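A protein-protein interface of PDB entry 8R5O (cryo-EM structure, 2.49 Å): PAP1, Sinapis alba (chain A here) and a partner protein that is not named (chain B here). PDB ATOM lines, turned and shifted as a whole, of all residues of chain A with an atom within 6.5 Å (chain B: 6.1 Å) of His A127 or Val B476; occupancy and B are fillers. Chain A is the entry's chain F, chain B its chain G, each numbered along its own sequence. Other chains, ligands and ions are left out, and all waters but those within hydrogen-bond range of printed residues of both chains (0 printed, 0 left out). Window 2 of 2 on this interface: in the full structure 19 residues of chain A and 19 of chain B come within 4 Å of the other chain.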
ATOM      1  N   LEU A 112     -10.423 -12.495  -1.621  1.00  0.00           N
ATOM      2  CA  LEU A 112     -10.827 -13.873  -1.874  1.00  0.00           C
ATOM      3  C   LEU A 112      -9.620 -14.759  -2.157  1.00  0.00           C
ATOM      4  O   LEU A 112      -9.565 -15.906  -1.700  1.00  0.00           O
ATOM      5  CB  LEU A 112     -11.818 -13.923  -3.035  1.00  0.00           C
ATOM      6  CG  LEU A 112     -12.537 -15.253  -3.262  1.00  0.00           C
ATOM      7  CD1 LEU A 112     -13.300 -15.663  -2.016  1.00  0.00           C
ATOM      8  CD2 LEU A 112     -13.470 -15.158  -4.457  1.00  0.00           C
ATOM      9  N   HIS A 116      -8.210 -17.972   0.514  1.00  0.00           N
ATOM     10  CA  HIS A 116      -7.854 -19.318   0.076  1.00  0.00           C
ATOM     11  C   HIS A 116      -6.365 -19.584   0.259  1.00  0.00           C
ATOM     12  O   HIS A 116      -5.971 -20.668   0.701  1.00  0.00           O
ATOM     13  CB  HIS A 116      -8.252 -19.521  -1.384  1.00  0.00           C
ATOM     14  CG  HIS A 116      -9.712 -19.779  -1.584  1.00  0.00           C
ATOM     15  ND1 HIS A 116     -10.277 -21.023  -1.410  1.00  0.00           N
ATOM     16  CD2 HIS A 116     -10.720 -18.957  -1.956  1.00  0.00           C
ATOM     17  CE1 HIS A 116     -11.571 -20.955  -1.661  1.00  0.00           C
ATOM     18  NE2 HIS A 116     -11.866 -19.712  -1.993  1.00  0.00           N
ATOM     19  N   GLU A 122      -4.572 -24.209  -2.938  1.00  0.00           N
ATOM     20  CA  GLU A 122      -4.092 -23.752  -4.234  1.00  0.00           C
ATOM     21  C   GLU A 122      -5.179 -23.785  -5.299  1.00  0.00           C
ATOM     22  O   GLU A 122      -5.187 -22.933  -6.195  1.00  0.00           O
ATOM     23  CB  GLU A 122      -2.896 -24.597  -4.673  1.00  0.00           C
ATOM     24  CG  GLU A 122      -2.045 -23.959  -5.754  1.00  0.00           C
ATOM     25  CD  GLU A 122      -0.754 -24.712  -5.994  1.00  0.00           C
ATOM     26  OE1 GLU A 122      -0.619 -25.842  -5.480  1.00  0.00           O
ATOM     27  OE2 GLU A 122       0.130 -24.172  -6.692  1.00  0.00           O
ATOM     28  N   GLN A 123      -6.098 -24.751  -5.223  1.00  0.00           N
ATOM     29  CA  GLN A 123      -7.132 -24.866  -6.246  1.00  0.00           C
ATOM     30  C   GLN A 123      -8.187 -23.777  -6.095  1.00  0.00           C
ATOM     31  O   GLN A 123      -8.624 -23.187  -7.090  1.00  0.00           O
ATOM     32  CB  GLN A 123      -7.776 -26.250  -6.184  1.00  0.00           C
ATOM     33  CG  GLN A 123      -6.808 -27.370  -5.835  1.00  0.00           C
ATOM     34  CD  GLN A 123      -5.627 -27.448  -6.782  1.00  0.00           C
ATOM     35  OE1 GLN A 123      -5.761 -27.224  -7.984  1.00  0.00           O
ATOM     36  NE2 GLN A 123      -4.456 -27.764  -6.239  1.00  0.00           N
ATOM     37  N   GLY A 124      -8.610 -23.499  -4.861  1.00  0.00           N
ATOM     38  CA  GLY A 124      -9.578 -22.437  -4.646  1.00  0.00           C
ATOM     39  C   GLY A 124      -9.015 -21.064  -4.961  1.00  0.00           C
ATOM     40  O   GLY A 124      -9.714 -20.209  -5.512  1.00  0.00           O
ATOM     41  N   ALA A 125      -7.748 -20.833  -4.612  1.00  0.00           N
ATOM     42  CA  ALA A 125      -7.114 -19.555  -4.916  1.00  0.00           C
ATOM     43  C   ALA A 125      -6.973 -19.352  -6.418  1.00  0.00           C
ATOM     44  O   ALA A 125      -7.162 -18.238  -6.920  1.00  0.00           O
ATOM     45  CB  ALA A 125      -5.754 -19.470  -4.227  1.00  0.00           C
ATOM     46  N   MET A 126      -6.635 -20.413  -7.153  1.00  0.00           N
ATOM     47  CA  MET A 126      -6.588 -20.319  -8.608  1.00  0.00           C
ATOM     48  C   MET A 126      -7.981 -20.106  -9.186  1.00  0.00           C
ATOM     49  O   MET A 126      -8.148 -19.375 -10.170  1.00  0.00           O
ATOM     50  CB  MET A 126      -5.946 -21.575  -9.195  1.00  0.00           C
ATOM     51  CG  MET A 126      -5.775 -21.535 -10.701  1.00  0.00           C
ATOM     52  SD  MET A 126      -4.730 -20.171 -11.241  1.00  0.00           S
ATOM     53  CE  MET A 126      -4.827 -20.358 -13.020  1.00  0.00           C
ATOM     54  N   HIS A 127      -8.992 -20.745  -8.594  1.00  0.00           N
ATOM     55  CA  HIS A 127     -10.369 -20.513  -9.016  1.00  0.00           C
ATOM     56  C   HIS A 127     -10.794 -19.076  -8.745  1.00  0.00           C
ATOM     57  O   HIS A 127     -11.509 -18.472  -9.552  1.00  0.00           O
ATOM     58  CB  HIS A 127     -11.303 -21.494  -8.308  1.00  0.00           C
ATOM     59  CG  HIS A 127     -12.755 -21.249  -8.579  1.00  0.00           C
ATOM     60  ND1 HIS A 127     -13.344 -21.539  -9.790  1.00  0.00           N
ATOM     61  CD2 HIS A 127     -13.735 -20.745  -7.794  1.00  0.00           C
ATOM     62  CE1 HIS A 127     -14.625 -21.222  -9.740  1.00  0.00           C
ATOM     63  NE2 HIS A 127     -14.888 -20.739  -8.539  1.00  0.00           N
ATOM     64  N   SER A 128     -10.366 -18.514  -7.611  1.00  0.00           N
ATOM     65  CA  SER A 128     -10.676 -17.122  -7.308  1.00  0.00           C
ATOM     66  C   SER A 128     -10.038 -16.180  -8.321  1.00  0.00           C
ATOM     67  O   SER A 128     -10.631 -15.161  -8.691  1.00  0.00           O
ATOM     68  CB  SER A 128     -10.213 -16.779  -5.893  1.00  0.00           C
ATOM     69  OG  SER A 128     -10.816 -17.640  -4.942  1.00  0.00           O
ATOM     70  N   LEU A 129      -8.824 -16.501  -8.776  1.00  0.00           N
ATOM     71  CA  LEU A 129      -8.183 -15.692  -9.807  1.00  0.00           C
ATOM     72  C   LEU A 129      -8.967 -15.742 -11.112  1.00  0.00           C
ATOM     73  O   LEU A 129      -9.078 -14.733 -11.817  1.00  0.00           O
ATOM     74  CB  LEU A 129      -6.745 -16.163 -10.027  1.00  0.00           C
ATOM     75  CG  LEU A 129      -5.978 -15.460 -11.150  1.00  0.00           C
ATOM     76  CD1 LEU A 129      -5.764 -13.992 -10.819  1.00  0.00           C
ATOM     77  CD2 LEU A 129      -4.655 -16.155 -11.427  1.00  0.00           C
ATOM     78  N   ARG A 130      -9.511 -16.912 -11.453  1.00  0.00           N
ATOM     79  CA  ARG A 130     -10.315 -17.031 -12.665  1.00  0.00           C
ATOM     80  C   ARG A 130     -11.597 -16.216 -12.558  1.00  0.00           C
ATOM     81  O   ARG A 130     -12.062 -15.646 -13.552  1.00  0.00           O
ATOM     82  CB  ARG A 130     -10.623 -18.501 -12.940  1.00  0.00           C
ATOM     83  CG  ARG A 130      -9.391 -19.314 -13.292  1.00  0.00           C
ATOM     84  CD  ARG A 130      -9.647 -20.804 -13.190  1.00  0.00           C
ATOM     85  NE  ARG A 130      -8.463 -21.573 -13.552  1.00  0.00           N
ATOM     86  CZ  ARG A 130      -8.336 -22.881 -13.382  1.00  0.00           C
ATOM     87  NH1 ARG A 130      -9.300 -23.603 -12.836  1.00  0.00           N
ATOM     88  NH2 ARG A 130      -7.214 -23.480 -13.770  1.00  0.00           N
ATOM     89  N   LYS A 131     -12.185 -16.154 -11.361  1.00  0.00           N
ATOM     90  CA  LYS A 131     -13.333 -15.281 -11.141  1.00  0.00           C
ATOM     91  C   LYS A 131     -12.967 -13.822 -11.375  1.00  0.00           C
ATOM     92  O   LYS A 131     -13.728 -13.075 -11.999  1.00  0.00           O
ATOM     93  CB  LYS A 131     -13.869 -15.470  -9.724  1.00  0.00           C
ATOM     94  CG  LYS A 131     -14.948 -16.523  -9.583  1.00  0.00           C
ATOM     95  CD  LYS A 131     -15.252 -16.775  -8.116  1.00  0.00           C
ATOM     96  CE  LYS A 131     -16.605 -17.433  -7.927  1.00  0.00           C
ATOM     97  NZ  LYS A 131     -17.719 -16.506  -8.268  1.00  0.00           N
ATOM     98  N   GLU A 132     -11.805 -13.398 -10.874  1.00  0.00           N
ATOM     99  CA  GLU A 132     -11.377 -12.012 -11.043  1.00  0.00           C
ATOM    100  C   GLU A 132     -11.139 -11.686 -12.511  1.00  0.00           C
ATOM    101  O   GLU A 132     -11.570 -10.639 -13.004  1.00  0.00           O
ATOM    102  CB  GLU A 132     -10.114 -11.759 -10.219  1.00  0.00           C
ATOM    103  CG  GLU A 132      -9.631 -10.323 -10.232  1.00  0.00           C
ATOM    104  CD  GLU A 132      -8.519 -10.078  -9.232  1.00  0.00           C
ATOM    105  OE1 GLU A 132      -7.938 -11.065  -8.733  1.00  0.00           O
ATOM    106  OE2 GLU A 132      -8.232  -8.901  -8.935  1.00  0.00           O
ATOM    107  N   GLY A 134     -12.416 -13.373 -15.055  1.00  0.00           N
ATOM    108  CA  GLY A 134     -13.705 -13.490 -15.713  1.00  0.00           C
ATOM    109  C   GLY A 134     -14.631 -12.322 -15.464  1.00  0.00           C
ATOM    110  O   GLY A 134     -15.544 -12.086 -16.261  1.00  0.00           O
ATOM    111  N   ARG B 440     -19.384 -28.824  -7.999  1.00  0.00           N
ATOM    112  CA  ARG B 440     -18.079 -28.204  -7.793  1.00  0.00           C
ATOM    113  C   ARG B 440     -17.113 -29.163  -7.107  1.00  0.00           C
ATOM    114  O   ARG B 440     -15.913 -29.162  -7.403  1.00  0.00           O
ATOM    115  CB  ARG B 440     -18.231 -26.918  -6.981  1.00  0.00           C
ATOM    116  CG  ARG B 440     -16.972 -26.067  -6.930  1.00  0.00           C
ATOM    117  CD  ARG B 440     -17.138 -24.851  -6.028  1.00  0.00           C
ATOM    118  NE  ARG B 440     -18.191 -23.950  -6.483  1.00  0.00           N
ATOM    119  CZ  ARG B 440     -19.388 -23.851  -5.920  1.00  0.00           C
ATOM    120  NH1 ARG B 440     -19.722 -24.583  -4.870  1.00  0.00           N
ATOM    121  NH2 ARG B 440     -20.272 -22.992  -6.420  1.00  0.00           N
ATOM    122  N   GLN B 444     -13.501 -30.563  -8.411  1.00  0.00           N
ATOM    123  CA  GLN B 444     -12.294 -30.459  -7.597  1.00  0.00           C
ATOM    124  C   GLN B 444     -11.691 -31.831  -7.326  1.00  0.00           C
ATOM    125  O   GLN B 444     -10.463 -31.981  -7.297  1.00  0.00           O
ATOM    126  CB  GLN B 444     -12.602 -29.737  -6.286  1.00  0.00           C
ATOM    127  CG  GLN B 444     -12.892 -28.251  -6.446  1.00  0.00           C
ATOM    128  CD  GLN B 444     -11.659 -27.445  -6.819  1.00  0.00           C
ATOM    129  OE1 GLN B 444     -10.534 -27.944  -6.763  1.00  0.00           O
ATOM    130  NE2 GLN B 444     -11.867 -26.190  -7.200  1.00  0.00           N
ATOM    131  N   TYR B 471     -24.338 -17.100 -12.567  1.00  0.00           N
ATOM    132  CA  TYR B 471     -23.781 -16.869 -13.893  1.00  0.00           C
ATOM    133  C   TYR B 471     -22.270 -16.681 -13.852  1.00  0.00           C
ATOM    134  O   TYR B 471     -21.574 -17.088 -14.789  1.00  0.00           O
ATOM    135  CB  TYR B 471     -24.451 -15.655 -14.533  1.00  0.00           C
ATOM    136  CG  TYR B 471     -25.959 -15.699 -14.463  1.00  0.00           C
ATOM    137  CD1 TYR B 471     -26.692 -16.464 -15.360  1.00  0.00           C
ATOM    138  CD2 TYR B 471     -26.650 -14.980 -13.497  1.00  0.00           C
ATOM    139  CE1 TYR B 471     -28.069 -16.510 -15.298  1.00  0.00           C
ATOM    140  CE2 TYR B 471     -28.028 -15.020 -13.430  1.00  0.00           C
ATOM    141  CZ  TYR B 471     -28.732 -15.786 -14.333  1.00  0.00           C
ATOM    142  OH  TYR B 471     -30.105 -15.830 -14.271  1.00  0.00           O
ATOM    143  N   GLU B 472     -21.749 -16.067 -12.789  1.00  0.00           N
ATOM    144  CA  GLU B 472     -20.307 -15.858 -12.695  1.00  0.00           C
ATOM    145  C   GLU B 472     -19.558 -17.182 -12.634  1.00  0.00           C
ATOM    146  O   GLU B 472     -18.550 -17.364 -13.324  1.00  0.00           O
ATOM    147  CB  GLU B 472     -19.978 -14.994 -11.478  1.00  0.00           C
ATOM    148  CG  GLU B 472     -19.928 -13.507 -11.777  1.00  0.00           C
ATOM    149  CD  GLU B 472     -21.249 -12.968 -12.287  1.00  0.00           C
ATOM    150  OE1 GLU B 472     -22.274 -13.159 -11.602  1.00  0.00           O
ATOM    151  OE2 GLU B 472     -21.261 -12.362 -13.379  1.00  0.00           O
ATOM    152  N   GLU B 473     -20.043 -18.124 -11.824  1.00  0.00           N
ATOM    153  CA  GLU B 473     -19.378 -19.417 -11.723  1.00  0.00           C
ATOM    154  C   GLU B 473     -19.631 -20.280 -12.953  1.00  0.00           C
ATOM    155  O   GLU B 473     -18.818 -21.155 -13.271  1.00  0.00           O
ATOM    156  CB  GLU B 473     -19.827 -20.138 -10.455  1.00  0.00           C
ATOM    157  CG  GLU B 473     -19.415 -19.426  -9.177  1.00  0.00           C
ATOM    158  CD  GLU B 473     -19.999 -20.064  -7.932  1.00  0.00           C
ATOM    159  OE1 GLU B 473     -20.919 -20.898  -8.066  1.00  0.00           O
ATOM    160  OE2 GLU B 473     -19.538 -19.733  -6.820  1.00  0.00           O
ATOM    161  N   ALA B 474     -20.746 -20.055 -13.652  1.00  0.00           N
ATOM    162  CA  ALA B 474     -21.010 -20.798 -14.880  1.00  0.00           C
ATOM    163  C   ALA B 474     -20.058 -20.383 -15.994  1.00  0.00           C
ATOM    164  O   ALA B 474     -19.544 -21.233 -16.728  1.00  0.00           O
ATOM    165  CB  ALA B 474     -22.460 -20.597 -15.316  1.00  0.00           C
ATOM    166  N   LEU B 475     -19.811 -19.079 -16.134  1.00  0.00           N
ATOM    167  CA  LEU B 475     -18.915 -18.598 -17.178  1.00  0.00           C
ATOM    168  C   LEU B 475     -17.451 -18.869 -16.856  1.00  0.00           C
ATOM    169  O   LEU B 475     -16.622 -18.879 -17.770  1.00  0.00           O
ATOM    170  CB  LEU B 475     -19.135 -17.104 -17.409  1.00  0.00           C
ATOM    171  CG  LEU B 475     -20.514 -16.737 -17.959  1.00  0.00           C
ATOM    172  CD1 LEU B 475     -20.698 -15.231 -18.017  1.00  0.00           C
ATOM    173  CD2 LEU B 475     -20.715 -17.356 -19.332  1.00  0.00           C
ATOM    174  N   VAL B 476     -17.115 -19.082 -15.583  1.00  0.00           N
ATOM    175  CA  VAL B 476     -15.767 -19.519 -15.238  1.00  0.00           C
ATOM    176  C   VAL B 476     -15.528 -20.937 -15.744  1.00  0.00           C
ATOM    177  O   VAL B 476     -14.484 -21.236 -16.335  1.00  0.00           O
ATOM    178  CB  VAL B 476     -15.538 -19.415 -13.719  1.00  0.00           C
ATOM    179  CG1 VAL B 476     -14.285 -20.170 -13.318  1.00  0.00           C
ATOM    180  CG2 VAL B 476     -15.431 -17.961 -13.305  1.00  0.00           C
ATOM    181  N   ALA B 477     -16.498 -21.827 -15.522  1.00  0.00           N
ATOM    182  CA  ALA B 477     -16.386 -23.189 -16.033  1.00  0.00           C
ATOM    183  C   ALA B 477     -16.326 -23.199 -17.554  1.00  0.00           C
ATOM    184  O   ALA B 477     -15.553 -23.959 -18.146  1.00  0.00           O
ATOM    185  CB  ALA B 477     -17.556 -24.034 -15.536  1.00  0.00           C
ATOM    186  N   PHE B 478     -17.133 -22.355 -18.202  1.00  0.00           N
ATOM    187  CA  PHE B 478     -17.072 -22.237 -19.655  1.00  0.00           C
ATOM    188  C   PHE B 478     -15.702 -21.750 -20.103  1.00  0.00           C
ATOM    189  O   PHE B 478     -15.161 -22.228 -21.108  1.00  0.00           O
ATOM    190  CB  PHE B 478     -18.171 -21.297 -20.147  1.00  0.00           C
ATOM    191  CG  PHE B 478     -18.289 -21.229 -21.642  1.00  0.00           C
ATOM    192  CD1 PHE B 478     -18.853 -22.274 -22.353  1.00  0.00           C
ATOM    193  CD2 PHE B 478     -17.848 -20.116 -22.334  1.00  0.00           C
ATOM    194  CE1 PHE B 478     -18.966 -22.215 -23.728  1.00  0.00           C
ATOM    195  CE2 PHE B 478     -17.958 -20.050 -23.708  1.00  0.00           C
ATOM    196  CZ  PHE B 478     -18.517 -21.100 -24.406  1.00  0.00           C
ATOM    197  N   ASN B 479     -15.128 -20.795 -19.372  1.00  0.00           N
ATOM    198  CA  ASN B 479     -13.773 -20.340 -19.665  1.00  0.00           C
ATOM    199  C   ASN B 479     -12.753 -21.448 -19.433  1.00  0.00           C
ATOM    200  O   ASN B 479     -11.791 -21.583 -20.198  1.00  0.00           O
ATOM    201  CB  ASN B 479     -13.440 -19.116 -18.813  1.00  0.00           C
ATOM    202  CG  ASN B 479     -13.956 -17.829 -19.420  1.00  0.00           C
ATOM    203  OD1 ASN B 479     -14.001 -17.681 -20.641  1.00  0.00           O
ATOM    204  ND2 ASN B 479     -14.343 -16.887 -18.570  1.00  0.00           N
ATOM    205  N   THR B 480     -12.941 -22.247 -18.381  1.00  0.00           N
ATOM    206  CA  THR B 480     -11.995 -23.311 -18.064  1.00  0.00           C
ATOM    207  C   THR B 480     -12.043 -24.453 -19.073  1.00  0.00           C
ATOM    208  O   THR B 480     -11.069 -25.207 -19.180  1.00  0.00           O
ATOM    209  CB  THR B 480     -12.263 -23.843 -16.654  1.00  0.00           C
ATOM    210  OG1 THR B 480     -12.512 -22.744 -15.771  1.00  0.00           O
ATOM    211  CG2 THR B 480     -11.066 -24.624 -16.136  1.00  0.00           C
ATOM    212  N   MET B 481     -13.143 -24.594 -19.817  1.00  0.00           N
ATOM    213  CA  MET B 481     -13.219 -25.645 -20.830  1.00  0.00           C
ATOM    214  C   MET B 481     -12.146 -25.464 -21.893  1.00  0.00           C
ATOM    215  O   MET B 481     -11.496 -26.433 -22.303  1.00  0.00           O
ATOM    216  CB  MET B 481     -14.603 -25.659 -21.477  1.00  0.00           C
ATOM    217  CG  MET B 481     -15.732 -26.001 -20.532  1.00  0.00           C
ATOM    218  SD  MET B 481     -17.311 -26.217 -21.374  1.00  0.00           S
ATOM    219  CE  MET B 481     -17.023 -27.751 -22.246  1.00  0.00           C
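The side-chain carboxylate (OE1) of Glu B473 is in salt-bridge range of the guanidinium group (NH2) of Arg B440, at 2.7 Å.
The backbone carbonyl oxygen of Val B476 lies within hydrogen-bond range of the side-chain hydroxyl of Thr B480.
Of the 14 printed residues of chain A, 4 touch a printed residue of chain B.
Printed residues of chain A that touch a printed residue of chain B: Gln A123, His A127, Arg A130 and Lys A131.
Hydrophobic or aromatic side chains of chain B that line the printed part of chain A: Val B476.
OE2 of Glu B473 is in salt-bridge range of NZ of Lys A131.
His A127 touches one residue of chain B.
Of the printed residues of chain B, Arg A130 touches Thr B480.
Of the printed residues of chain B, Lys A131 touches Glu B473.
Printed residues of chain A within 4 Å of Glu B473: Lys A131 (3.5 Å).
Of the printed residues of chain A, Val B476 touches His A127.
Printed residues of chain A within 4 Å of Thr B480: Arg A130.
The nearest residue of chain B that does not touch His A127 is Glu B473 (4.8 Å).
The nearest printed residue of chain A that does not touch Val B476 is Lys A131 (4.02 Å).
The nearest printed residue of chain B that does not touch Lys A131 is Val B476 (4.02 Å).
Among the printed residues, merely in contact across the chains: Gln A123 with Gln B444 (3.3 Å), His A127 with Val B476 (3.7 Å) and Arg A130 with Thr B480 (3.9 Å).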
